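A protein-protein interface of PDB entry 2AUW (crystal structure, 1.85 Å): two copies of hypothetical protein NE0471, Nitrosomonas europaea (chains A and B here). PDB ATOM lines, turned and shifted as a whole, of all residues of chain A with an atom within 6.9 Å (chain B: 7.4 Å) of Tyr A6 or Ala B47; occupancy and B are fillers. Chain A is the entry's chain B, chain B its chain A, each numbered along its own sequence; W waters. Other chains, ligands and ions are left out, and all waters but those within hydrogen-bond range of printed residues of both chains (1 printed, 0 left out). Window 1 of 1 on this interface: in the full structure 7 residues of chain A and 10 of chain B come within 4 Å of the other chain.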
ATOM      1  N   ASN A   4     -17.263   2.785  -0.957  1.00  0.00           N
ATOM      2  CA  ASN A   4     -16.363   1.660  -1.139  1.00  0.00           C
ATOM      3  C   ASN A   4     -15.292   2.060  -2.115  1.00  0.00           C
ATOM      4  O   ASN A   4     -15.439   3.042  -2.835  1.00  0.00           O
ATOM      5  CB  ASN A   4     -17.128   0.427  -1.615  1.00  0.00           C
ATOM      6  CG  ASN A   4     -18.049  -0.121  -0.539  1.00  0.00           C
ATOM      7  OD1 ASN A   4     -17.585  -0.644   0.465  1.00  0.00           O
ATOM      8  ND2 ASN A   4     -19.353   0.033  -0.730  1.00  0.00           N
ATOM      9  N   GLU A   5     -14.163   1.371  -2.134  1.00  0.00           N
ATOM     10  CA  GLU A   5     -13.160   1.871  -3.062  1.00  0.00           C
ATOM     11  C   GLU A   5     -12.807   0.952  -4.235  1.00  0.00           C
ATOM     12  O   GLU A   5     -12.952  -0.288  -4.179  1.00  0.00           O
ATOM     13  CB  GLU A   5     -11.948   2.505  -2.367  1.00  0.00           C
ATOM     14  CG  GLU A   5     -11.194   3.490  -3.280  1.00  0.00           C
ATOM     15  CD  GLU A   5     -10.784   4.790  -2.594  1.00  0.00           C
ATOM     16  OE1 GLU A   5     -10.829   5.847  -3.267  1.00  0.00           O
ATOM     17  OE2 GLU A   5     -10.422   4.769  -1.397  1.00  0.00           O
ATOM     18  N   TYR A   6     -12.454   1.614  -5.324  1.00  0.00           N
ATOM     19  CA  TYR A   6     -12.048   1.003  -6.582  1.00  0.00           C
ATOM     20  C   TYR A   6     -10.813   1.805  -6.962  1.00  0.00           C
ATOM     21  O   TYR A   6     -10.847   3.026  -6.920  1.00  0.00           O
ATOM     22  CB  TYR A   6     -13.104   1.161  -7.684  1.00  0.00           C
ATOM     23  CG  TYR A   6     -12.683   0.545  -9.018  1.00  0.00           C
ATOM     24  CD1 TYR A   6     -12.333  -0.792  -9.094  1.00  0.00           C
ATOM     25  CD2 TYR A   6     -12.651   1.305 -10.188  1.00  0.00           C
ATOM     26  CE1 TYR A   6     -11.936  -1.370 -10.297  1.00  0.00           C
ATOM     27  CE2 TYR A   6     -12.261   0.733 -11.417  1.00  0.00           C
ATOM     28  CZ  TYR A   6     -11.905  -0.617 -11.446  1.00  0.00           C
ATOM     29  OH  TYR A   6     -11.519  -1.240 -12.612  1.00  0.00           O
ATOM     30  N   PHE A   7      -9.742   1.094  -7.282  1.00  0.00           N
ATOM     31  CA  PHE A   7      -8.518   1.638  -7.865  1.00  0.00           C
ATOM     32  C   PHE A   7      -8.293   0.976  -9.233  1.00  0.00           C
ATOM     33  O   PHE A   7      -8.077  -0.255  -9.376  1.00  0.00           O
ATOM     34  CB  PHE A   7      -7.322   1.470  -6.897  1.00  0.00           C
ATOM     35  CG  PHE A   7      -6.006   2.016  -7.424  1.00  0.00           C
ATOM     36  CD1 PHE A   7      -5.766   3.392  -7.496  1.00  0.00           C
ATOM     37  CD2 PHE A   7      -4.994   1.140  -7.825  1.00  0.00           C
ATOM     38  CE1 PHE A   7      -4.537   3.887  -8.004  1.00  0.00           C
ATOM     39  CE2 PHE A   7      -3.759   1.627  -8.318  1.00  0.00           C
ATOM     40  CZ  PHE A   7      -3.538   3.012  -8.403  1.00  0.00           C
ATOM     41  N   PHE A   8      -8.391   1.803 -10.249  1.00  0.00           N
ATOM     42  CA  PHE A   8      -8.392   1.316 -11.626  1.00  0.00           C
ATOM     43  C   PHE A   8      -7.017   0.709 -12.049  1.00  0.00           C
ATOM     44  O   PHE A   8      -6.956  -0.452 -12.450  1.00  0.00           O
ATOM     45  CB  PHE A   8      -8.915   2.403 -12.601  1.00  0.00           C
ATOM     46  CG  PHE A   8      -8.721   2.036 -14.066  1.00  0.00           C
ATOM     47  CD1 PHE A   8      -9.610   1.156 -14.699  1.00  0.00           C
ATOM     48  CD2 PHE A   8      -7.620   2.513 -14.781  1.00  0.00           C
ATOM     49  CE1 PHE A   8      -9.420   0.771 -16.044  1.00  0.00           C
ATOM     50  CE2 PHE A   8      -7.411   2.151 -16.116  1.00  0.00           C
ATOM     51  CZ  PHE A   8      -8.324   1.275 -16.761  1.00  0.00           C
ATOM     52  N   PRO A   9      -5.907   1.450 -11.893  1.00  0.00           N
ATOM     53  CA  PRO A   9      -4.624   0.869 -12.380  1.00  0.00           C
ATOM     54  C   PRO A   9      -4.195  -0.444 -11.709  1.00  0.00           C
ATOM     55  O   PRO A   9      -4.425  -0.665 -10.504  1.00  0.00           O
ATOM     56  CB  PRO A   9      -3.595   1.976 -12.058  1.00  0.00           C
ATOM     57  CG  PRO A   9      -4.401   3.210 -11.929  1.00  0.00           C
ATOM     58  CD  PRO A   9      -5.691   2.780 -11.298  1.00  0.00           C
ATOM     59  N   LYS A  10      -3.587  -1.334 -12.493  1.00  0.00           N
ATOM     60  CA  LYS A  10      -3.005  -2.559 -11.955  1.00  0.00           C
ATOM     61  C   LYS A  10      -1.495  -2.398 -11.993  1.00  0.00           C
ATOM     62  O   LYS A  10      -0.962  -1.879 -12.955  1.00  0.00           O
ATOM     63  CB  LYS A  10      -3.381  -3.787 -12.813  1.00  0.00           C
ATOM     64  CG  LYS A  10      -4.877  -4.100 -12.826  1.00  0.00           C
ATOM     65  CD  LYS A  10      -5.238  -4.949 -14.066  1.00  0.00           C
ATOM     66  CE  LYS A  10      -6.719  -4.846 -14.415  1.00  0.00           C
ATOM     67  NZ  LYS A  10      -7.550  -5.887 -13.730  1.00  0.00           N
ATOM     68  N   ARG A  76      -0.580  -0.929  -3.534  1.00  0.00           N
ATOM     69  CA  ARG A  76      -0.257  -0.394  -4.876  1.00  0.00           C
ATOM     70  C   ARG A  76      -0.896   0.984  -5.091  1.00  0.00           C
ATOM     71  O   ARG A  76      -0.290   1.853  -5.704  1.00  0.00           O
ATOM     72  CB  ARG A  76      -0.630  -1.376  -6.011  1.00  0.00           C
ATOM     73  CG  ARG A  76      -2.112  -1.571  -6.191  1.00  0.00           C
ATOM     74  CD  ARG A  76      -2.352  -2.532  -7.314  1.00  0.00           C
ATOM     75  NE  ARG A  76      -3.578  -2.268  -8.081  1.00  0.00           N
ATOM     76  CZ  ARG A  76      -4.810  -2.611  -7.695  1.00  0.00           C
ATOM     77  NH1 ARG A  76      -5.859  -2.342  -8.482  1.00  0.00           N
ATOM     78  NH2 ARG A  76      -5.001  -3.200  -6.517  1.00  0.00           N
ATOM     79  N   HIS A  92      -5.054  10.836  -7.070  1.00  0.00           N
ATOM     80  CA  HIS A  92      -6.411  10.436  -6.691  1.00  0.00           C
ATOM     81  C   HIS A  92      -6.652  10.473  -5.163  1.00  0.00           C
ATOM     82  O   HIS A  92      -7.788  10.670  -4.730  1.00  0.00           O
ATOM     83  CB  HIS A  92      -6.713   9.026  -7.233  1.00  0.00           C
ATOM     84  CG  HIS A  92      -6.025   7.937  -6.480  1.00  0.00           C
ATOM     85  ND1 HIS A  92      -4.690   7.648  -6.647  1.00  0.00           N
ATOM     86  CD2 HIS A  92      -6.491   7.061  -5.554  1.00  0.00           C
ATOM     87  CE1 HIS A  92      -4.357   6.649  -5.849  1.00  0.00           C
ATOM     88  NE2 HIS A  92      -5.434   6.275  -5.173  1.00  0.00           N
ATOM     89  N   SER A 121     -15.967  10.251 -10.295  1.00  0.00           N
ATOM     90  CA  SER A 121     -15.570   8.857 -10.125  1.00  0.00           C
ATOM     91  C   SER A 121     -14.247   8.515 -10.839  1.00  0.00           C
ATOM     92  O   SER A 121     -13.375   7.883 -10.266  1.00  0.00           O
ATOM     93  CB  SER A 121     -16.669   7.942 -10.640  1.00  0.00           C
ATOM     94  OG  SER A 121     -16.298   6.591 -10.473  1.00  0.00           O
ATOM     95  N   ARG A 124     -11.476  10.025  -8.817  1.00  0.00           N
ATOM     96  CA  ARG A 124     -11.419   9.370  -7.515  1.00  0.00           C
ATOM     97  C   ARG A 124     -10.712   8.003  -7.596  1.00  0.00           C
ATOM     98  O   ARG A 124     -10.018   7.606  -6.669  1.00  0.00           O
ATOM     99  CB  ARG A 124     -12.866   9.160  -7.011  1.00  0.00           C
ATOM    100  CG  ARG A 124     -13.019   8.835  -5.554  1.00  0.00           C
ATOM    101  CD  ARG A 124     -14.470   8.479  -5.229  1.00  0.00           C
ATOM    102  NE  ARG A 124     -14.801   7.064  -5.466  1.00  0.00           N
ATOM    103  CZ  ARG A 124     -14.570   6.062  -4.605  1.00  0.00           C
ATOM    104  NH1 ARG A 124     -14.925   4.823  -4.924  1.00  0.00           N
ATOM    105  NH2 ARG A 124     -13.988   6.281  -3.429  1.00  0.00           N
ATOM    106  N   THR A 125     -10.981   7.262  -8.681  1.00  0.00           N
ATOM    107  CA  THR A 125     -10.557   5.867  -8.827  1.00  0.00           C
ATOM    108  C   THR A 125      -9.258   5.747  -9.659  1.00  0.00           C
ATOM    109  O   THR A 125      -8.834   4.649  -9.982  1.00  0.00           O
ATOM    110  CB  THR A 125     -11.648   5.051  -9.467  1.00  0.00           C
ATOM    111  OG1 THR A 125     -11.924   5.586 -10.772  1.00  0.00           O
ATOM    112  CG2 THR A 125     -12.913   5.076  -8.600  1.00  0.00           C
ATOM    113  N   ALA A 126      -8.660   6.891 -10.012  1.00  0.00           N
ATOM    114  CA  ALA A 126      -7.396   6.952 -10.800  1.00  0.00           C
ATOM    115  C   ALA A 126      -7.578   6.378 -12.211  1.00  0.00           C
ATOM    116  O   ALA A 126      -6.645   5.823 -12.789  1.00  0.00           O
ATOM    117  CB  ALA A 126      -6.214   6.255 -10.052  1.00  0.00           C
ATOM    118  N   HIS A 127      -8.798   6.489 -12.727  1.00  0.00           N
ATOM    119  CA  HIS A 127      -9.139   6.020 -14.084  1.00  0.00           C
ATOM    120  C   HIS A 127      -8.764   7.110 -15.098  1.00  0.00           C
ATOM    121  O   HIS A 127      -8.552   6.807 -16.267  1.00  0.00           O
ATOM    122  CB  HIS A 127     -10.637   5.645 -14.149  1.00  0.00           C
ATOM    123  CG  HIS A 127     -10.999   4.661 -15.245  1.00  0.00           C
ATOM    124  ND1 HIS A 127     -10.251   4.496 -16.396  1.00  0.00           N
ATOM    125  CD2 HIS A 127     -12.060   3.822 -15.371  1.00  0.00           C
ATOM    126  CE1 HIS A 127     -10.823   3.583 -17.173  1.00  0.00           C
ATOM    127  NE2 HIS A 127     -11.917   3.149 -16.567  1.00  0.00           N
ATOM    128  N   TYR B  20     -17.392  -9.876 -17.121  1.00  0.00           N
ATOM    129  CA  TYR B  20     -18.416  -9.629 -16.103  1.00  0.00           C
ATOM    130  C   TYR B  20     -19.702 -10.381 -16.451  1.00  0.00           C
ATOM    131  O   TYR B  20     -20.769  -9.796 -16.622  1.00  0.00           O
ATOM    132  CB  TYR B  20     -18.660  -8.128 -15.962  1.00  0.00           C
ATOM    133  CG  TYR B  20     -17.424  -7.403 -15.506  1.00  0.00           C
ATOM    134  CD1 TYR B  20     -17.107  -7.339 -14.164  1.00  0.00           C
ATOM    135  CD2 TYR B  20     -16.553  -6.826 -16.424  1.00  0.00           C
ATOM    136  CE1 TYR B  20     -15.971  -6.690 -13.724  1.00  0.00           C
ATOM    137  CE2 TYR B  20     -15.398  -6.176 -16.002  1.00  0.00           C
ATOM    138  CZ  TYR B  20     -15.119  -6.113 -14.657  1.00  0.00           C
ATOM    139  OH  TYR B  20     -13.985  -5.487 -14.224  1.00  0.00           O
ATOM    140  N   ILE B  39     -23.231  -2.280 -17.922  1.00  0.00           N
ATOM    141  CA  ILE B  39     -23.903  -1.452 -16.920  1.00  0.00           C
ATOM    142  C   ILE B  39     -22.937  -1.114 -15.772  1.00  0.00           C
ATOM    143  O   ILE B  39     -22.948   0.006 -15.276  1.00  0.00           O
ATOM    144  CB  ILE B  39     -25.257  -2.044 -16.425  1.00  0.00           C
ATOM    145  CG1 ILE B  39     -26.089  -0.954 -15.714  1.00  0.00           C
ATOM    146  CG2 ILE B  39     -25.052  -3.309 -15.607  1.00  0.00           C
ATOM    147  CD1 ILE B  39     -27.481  -1.431 -15.248  1.00  0.00           C
ATOM    148  N   LEU B  40     -22.084  -2.061 -15.390  1.00  0.00           N
ATOM    149  CA  LEU B  40     -21.106  -1.799 -14.298  1.00  0.00           C
ATOM    150  C   LEU B  40     -20.118  -0.698 -14.673  1.00  0.00           C
ATOM    151  O   LEU B  40     -19.730   0.082 -13.816  1.00  0.00           O
ATOM    152  CB  LEU B  40     -20.350  -3.059 -13.883  1.00  0.00           C
ATOM    153  CG  LEU B  40     -21.107  -4.232 -13.247  1.00  0.00           C
ATOM    154  CD1 LEU B  40     -20.147  -5.427 -13.116  1.00  0.00           C
ATOM    155  CD2 LEU B  40     -21.781  -3.868 -11.926  1.00  0.00           C
ATOM    156  N   ARG B  41     -19.733  -0.632 -15.953  1.00  0.00           N
ATOM    157  CA  ARG B  41     -18.871   0.459 -16.468  1.00  0.00           C
ATOM    158  C   ARG B  41     -19.599   1.789 -16.700  1.00  0.00           C
ATOM    159  O   ARG B  41     -18.984   2.874 -16.647  1.00  0.00           O
ATOM    160  CB  ARG B  41     -18.230   0.038 -17.778  1.00  0.00           C
ATOM    161  CG  ARG B  41     -17.151  -1.003 -17.632  1.00  0.00           C
ATOM    162  CD  ARG B  41     -16.503  -1.255 -18.972  1.00  0.00           C
ATOM    163  NE  ARG B  41     -17.396  -1.940 -19.898  1.00  0.00           N
ATOM    164  CZ  ARG B  41     -17.482  -3.259 -20.002  1.00  0.00           C
ATOM    165  NH1 ARG B  41     -16.716  -4.038 -19.243  1.00  0.00           N
ATOM    166  NH2 ARG B  41     -18.348  -3.797 -20.857  1.00  0.00           N
ATOM    167  N   ILE B  43     -22.475   3.000 -14.923  1.00  0.00           N
ATOM    168  CA  ILE B  43     -22.964   3.677 -13.729  1.00  0.00           C
ATOM    169  C   ILE B  43     -21.841   3.863 -12.718  1.00  0.00           C
ATOM    170  O   ILE B  43     -21.337   2.877 -12.193  1.00  0.00           O
ATOM    171  CB  ILE B  43     -24.140   2.906 -13.088  1.00  0.00           C
ATOM    172  CG1 ILE B  43     -25.220   2.595 -14.158  1.00  0.00           C
ATOM    173  CG2 ILE B  43     -24.691   3.667 -11.881  1.00  0.00           C
ATOM    174  CD1 ILE B  43     -26.472   1.825 -13.624  1.00  0.00           C
ATOM    175  N   PRO B  44     -21.455   5.126 -12.448  1.00  0.00           N
ATOM    176  CA  PRO B  44     -20.261   5.420 -11.631  1.00  0.00           C
ATOM    177  C   PRO B  44     -20.314   4.728 -10.275  1.00  0.00           C
ATOM    178  O   PRO B  44     -19.316   4.207  -9.799  1.00  0.00           O
ATOM    179  CB  PRO B  44     -20.350   6.925 -11.405  1.00  0.00           C
ATOM    180  CG  PRO B  44     -21.230   7.449 -12.467  1.00  0.00           C
ATOM    181  CD  PRO B  44     -22.142   6.347 -12.889  1.00  0.00           C
ATOM    182  N   ASP B  45     -21.494   4.744  -9.673  1.00  0.00           N
ATOM    183  CA  ASP B  45     -21.739   4.215  -8.334  1.00  0.00           C
ATOM    184  C   ASP B  45     -21.362   2.737  -8.220  1.00  0.00           C
ATOM    185  O   ASP B  45     -21.090   2.251  -7.121  1.00  0.00           O
ATOM    186  CB  ASP B  45     -23.221   4.403  -8.010  1.00  0.00           C
ATOM    187  CG  ASP B  45     -23.684   5.816  -8.260  1.00  0.00           C
ATOM    188  OD1 ASP B  45     -23.728   6.545  -7.254  1.00  0.00           O
ATOM    189  OD2 ASP B  45     -23.939   6.209  -9.448  1.00  0.00           O
ATOM    190  N   LEU B  46     -21.367   2.040  -9.363  1.00  0.00           N
ATOM    191  CA  LEU B  46     -21.107   0.611  -9.429  1.00  0.00           C
ATOM    192  C   LEU B  46     -19.619   0.298  -9.642  1.00  0.00           C
ATOM    193  O   LEU B  46     -19.246  -0.850  -9.787  1.00  0.00           O
ATOM    194  CB  LEU B  46     -21.957  -0.062 -10.539  1.00  0.00           C
ATOM    195  CG  LEU B  46     -23.501   0.076 -10.488  1.00  0.00           C
ATOM    196  CD1 LEU B  46     -24.148  -0.575 -11.722  1.00  0.00           C
ATOM    197  CD2 LEU B  46     -24.055  -0.571  -9.240  1.00  0.00           C
ATOM    198  N   ALA B  47     -18.783   1.336  -9.654  1.00  0.00           N
ATOM    199  CA  ALA B  47     -17.367   1.148  -9.962  1.00  0.00           C
ATOM    200  C   ALA B  47     -16.666   0.129  -9.044  1.00  0.00           C
ATOM    201  O   ALA B  47     -15.911  -0.671  -9.538  1.00  0.00           O
ATOM    202  CB  ALA B  47     -16.620   2.506 -10.011  1.00  0.00           C
ATOM    203  N   PRO B  48     -16.905   0.160  -7.717  1.00  0.00           N
ATOM    204  CA  PRO B  48     -16.242  -0.834  -6.858  1.00  0.00           C
ATOM    205  C   PRO B  48     -16.473  -2.278  -7.264  1.00  0.00           C
ATOM    206  O   PRO B  48     -15.659  -3.163  -6.942  1.00  0.00           O
ATOM    207  CB  PRO B  48     -16.803  -0.508  -5.464  1.00  0.00           C
ATOM    208  CG  PRO B  48     -17.037   0.962  -5.554  1.00  0.00           C
ATOM    209  CD  PRO B  48     -17.649   1.137  -6.903  1.00  0.00           C
ATOM    210  N   ILE B  49     -17.535  -2.524  -8.030  1.00  0.00           N
ATOM    211  CA  ILE B  49     -17.852  -3.889  -8.447  1.00  0.00           C
ATOM    212  C   ILE B  49     -16.993  -4.387  -9.613  1.00  0.00           C
ATOM    213  O   ILE B  49     -16.868  -5.592  -9.837  1.00  0.00           O
ATOM    214  CB  ILE B  49     -19.400  -4.051  -8.729  1.00  0.00           C
ATOM    215  CG1 ILE B  49     -20.204  -3.690  -7.463  1.00  0.00           C
ATOM    216  CG2 ILE B  49     -19.756  -5.471  -9.222  1.00  0.00           C
ATOM    217  CD1 ILE B  49     -21.715  -3.459  -7.696  1.00  0.00           C
ATOM    218  N   LEU B  50     -16.377  -3.461 -10.337  1.00  0.00           N
ATOM    219  CA  LEU B  50     -15.503  -3.828 -11.453  1.00  0.00           C
ATOM    220  C   LEU B  50     -14.228  -4.580 -11.011  1.00  0.00           C
ATOM    221  O   LEU B  50     -13.650  -5.353 -11.783  1.00  0.00           O
ATOM    222  CB  LEU B  50     -15.150  -2.594 -12.250  1.00  0.00           C
ATOM    223  CG  LEU B  50     -16.337  -2.022 -13.016  1.00  0.00           C
ATOM    224  CD1 LEU B  50     -15.993  -0.638 -13.474  1.00  0.00           C
ATOM    225  CD2 LEU B  50     -16.700  -2.922 -14.190  1.00  0.00           C
ATOM    226  N   ASP B  51     -13.828  -4.360  -9.763  1.00  0.00           N
ATOM    227  CA  ASP B  51     -12.723  -5.107  -9.146  1.00  0.00           C
ATOM    228  C   ASP B  51     -13.119  -6.575  -9.119  1.00  0.00           C
ATOM    229  O   ASP B  51     -14.096  -6.927  -8.449  1.00  0.00           O
ATOM    230  CB  ASP B  51     -12.451  -4.569  -7.735  1.00  0.00           C
ATOM    231  CG  ASP B  51     -11.581  -5.508  -6.871  1.00  0.00           C
ATOM    232  OD1 ASP B  51     -10.884  -6.403  -7.401  1.00  0.00           O
ATOM    233  OD2 ASP B  51     -11.598  -5.325  -5.635  1.00  0.00           O
ATOM    234  N   PRO B  52     -12.367  -7.428  -9.855  1.00  0.00           N
ATOM    235  CA  PRO B  52     -12.650  -8.856 -10.046  1.00  0.00           C
ATOM    236  C   PRO B  52     -12.869  -9.669  -8.765  1.00  0.00           C
ATOM    237  O   PRO B  52     -13.542 -10.698  -8.821  1.00  0.00           O
ATOM    238  CB  PRO B  52     -11.412  -9.368 -10.794  1.00  0.00           C
ATOM    239  CG  PRO B  52     -10.900  -8.162 -11.531  1.00  0.00           C
ATOM    240  CD  PRO B  52     -11.146  -7.019 -10.590  1.00  0.00           C
ATOM    241  N   ALA B  54     -14.316  -8.272  -5.930  1.00  0.00           N
ATOM    242  CA  ALA B  54     -15.631  -7.828  -5.472  1.00  0.00           C
ATOM    243  C   ALA B  54     -16.742  -8.384  -6.366  1.00  0.00           C
ATOM    244  O   ALA B  54     -17.808  -8.749  -5.857  1.00  0.00           O
ATOM    245  CB  ALA B  54     -15.705  -6.298  -5.395  1.00  0.00           C
ATOM    246  N   PHE B  70     -23.068  -5.297  -2.891  1.00  0.00           N
ATOM    247  CA  PHE B  70     -23.071  -4.496  -1.684  1.00  0.00           C
ATOM    248  C   PHE B  70     -24.503  -4.261  -1.259  1.00  0.00           C
ATOM    249  O   PHE B  70     -24.854  -4.592  -0.145  1.00  0.00           O
ATOM    250  CB  PHE B  70     -22.383  -3.148  -1.906  1.00  0.00           C
ATOM    251  CG  PHE B  70     -20.938  -3.270  -2.248  1.00  0.00           C
ATOM    252  CD1 PHE B  70     -20.528  -3.311  -3.585  1.00  0.00           C
ATOM    253  CD2 PHE B  70     -19.982  -3.368  -1.245  1.00  0.00           C
ATOM    254  CE1 PHE B  70     -19.202  -3.440  -3.914  1.00  0.00           C
ATOM    255  CE2 PHE B  70     -18.631  -3.500  -1.573  1.00  0.00           C
ATOM    256  CZ  PHE B  70     -18.249  -3.545  -2.896  1.00  0.00           C
HETATM  257  O   HOH W   1     -14.275  -2.750  -4.690  1.00  0.00           O
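The backbone carbonyl oxygen of Leu B50 sits at hydrogen-bond distance from the side-chain hydroxyl of Tyr B20. The backbone carbonyl oxygen of Asn A4 is in hydrogen-bond range of the guanidinium group of Arg A124 (2.8 Å). O of Ser A121 is in hydrogen-bond range of OG1 of Thr A125 (2.8 Å).
Among the printed residues, merely in contact across the chains: Tyr A6 with Ala B47, Asn A4 with Phe B70, Tyr A6 with Asp B51, Asn A4 with Pro B48, Tyr A6 with Pro B48, Tyr A6 with Leu B50 and Ser A121 with Pro B44.
Printed residues of chain B within 4 Å of Ser A121: Pro B44. Of the printed residues of chain A, Pro B44 touches Ser A121 (3.9 Å). Ala B47 touches one residue of chain A. Of the printed residues of chain A, Leu B50 touches Tyr A6 (3.9 Å). Printed residues of chain A within 4 Å of Asp B51: Tyr A6 (3.6 Å). Of the printed residues of chain A, Phe B70 touches Asn A4. The nearest residue of chain B that does not touch Tyr A6 is Tyr B20 (5.2 Å). The nearest printed residue of chain B that does not touch Asn A4 is Ala B47 (7.0 Å).
Of the 14 printed residues of chain A, 3 touch a printed residue of chain B. Hydrophobic or aromatic side chains of chain B within 4 Å of the printed part of chain A: Pro B44, Pro B48, Leu B50 and Phe B70. Among the printed residues, 7 pairs touch across the chains. Among the printed residues, no Asp or Glu carboxylate lies within 4 Å of a Lys or Arg side-chain nitrogen of the other chain.
No position is printed for both chains.
Water W1 bridges the backbone carbonyl oxygen of Pro B48 and the backbone carbonyl oxygen of Glu A5.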
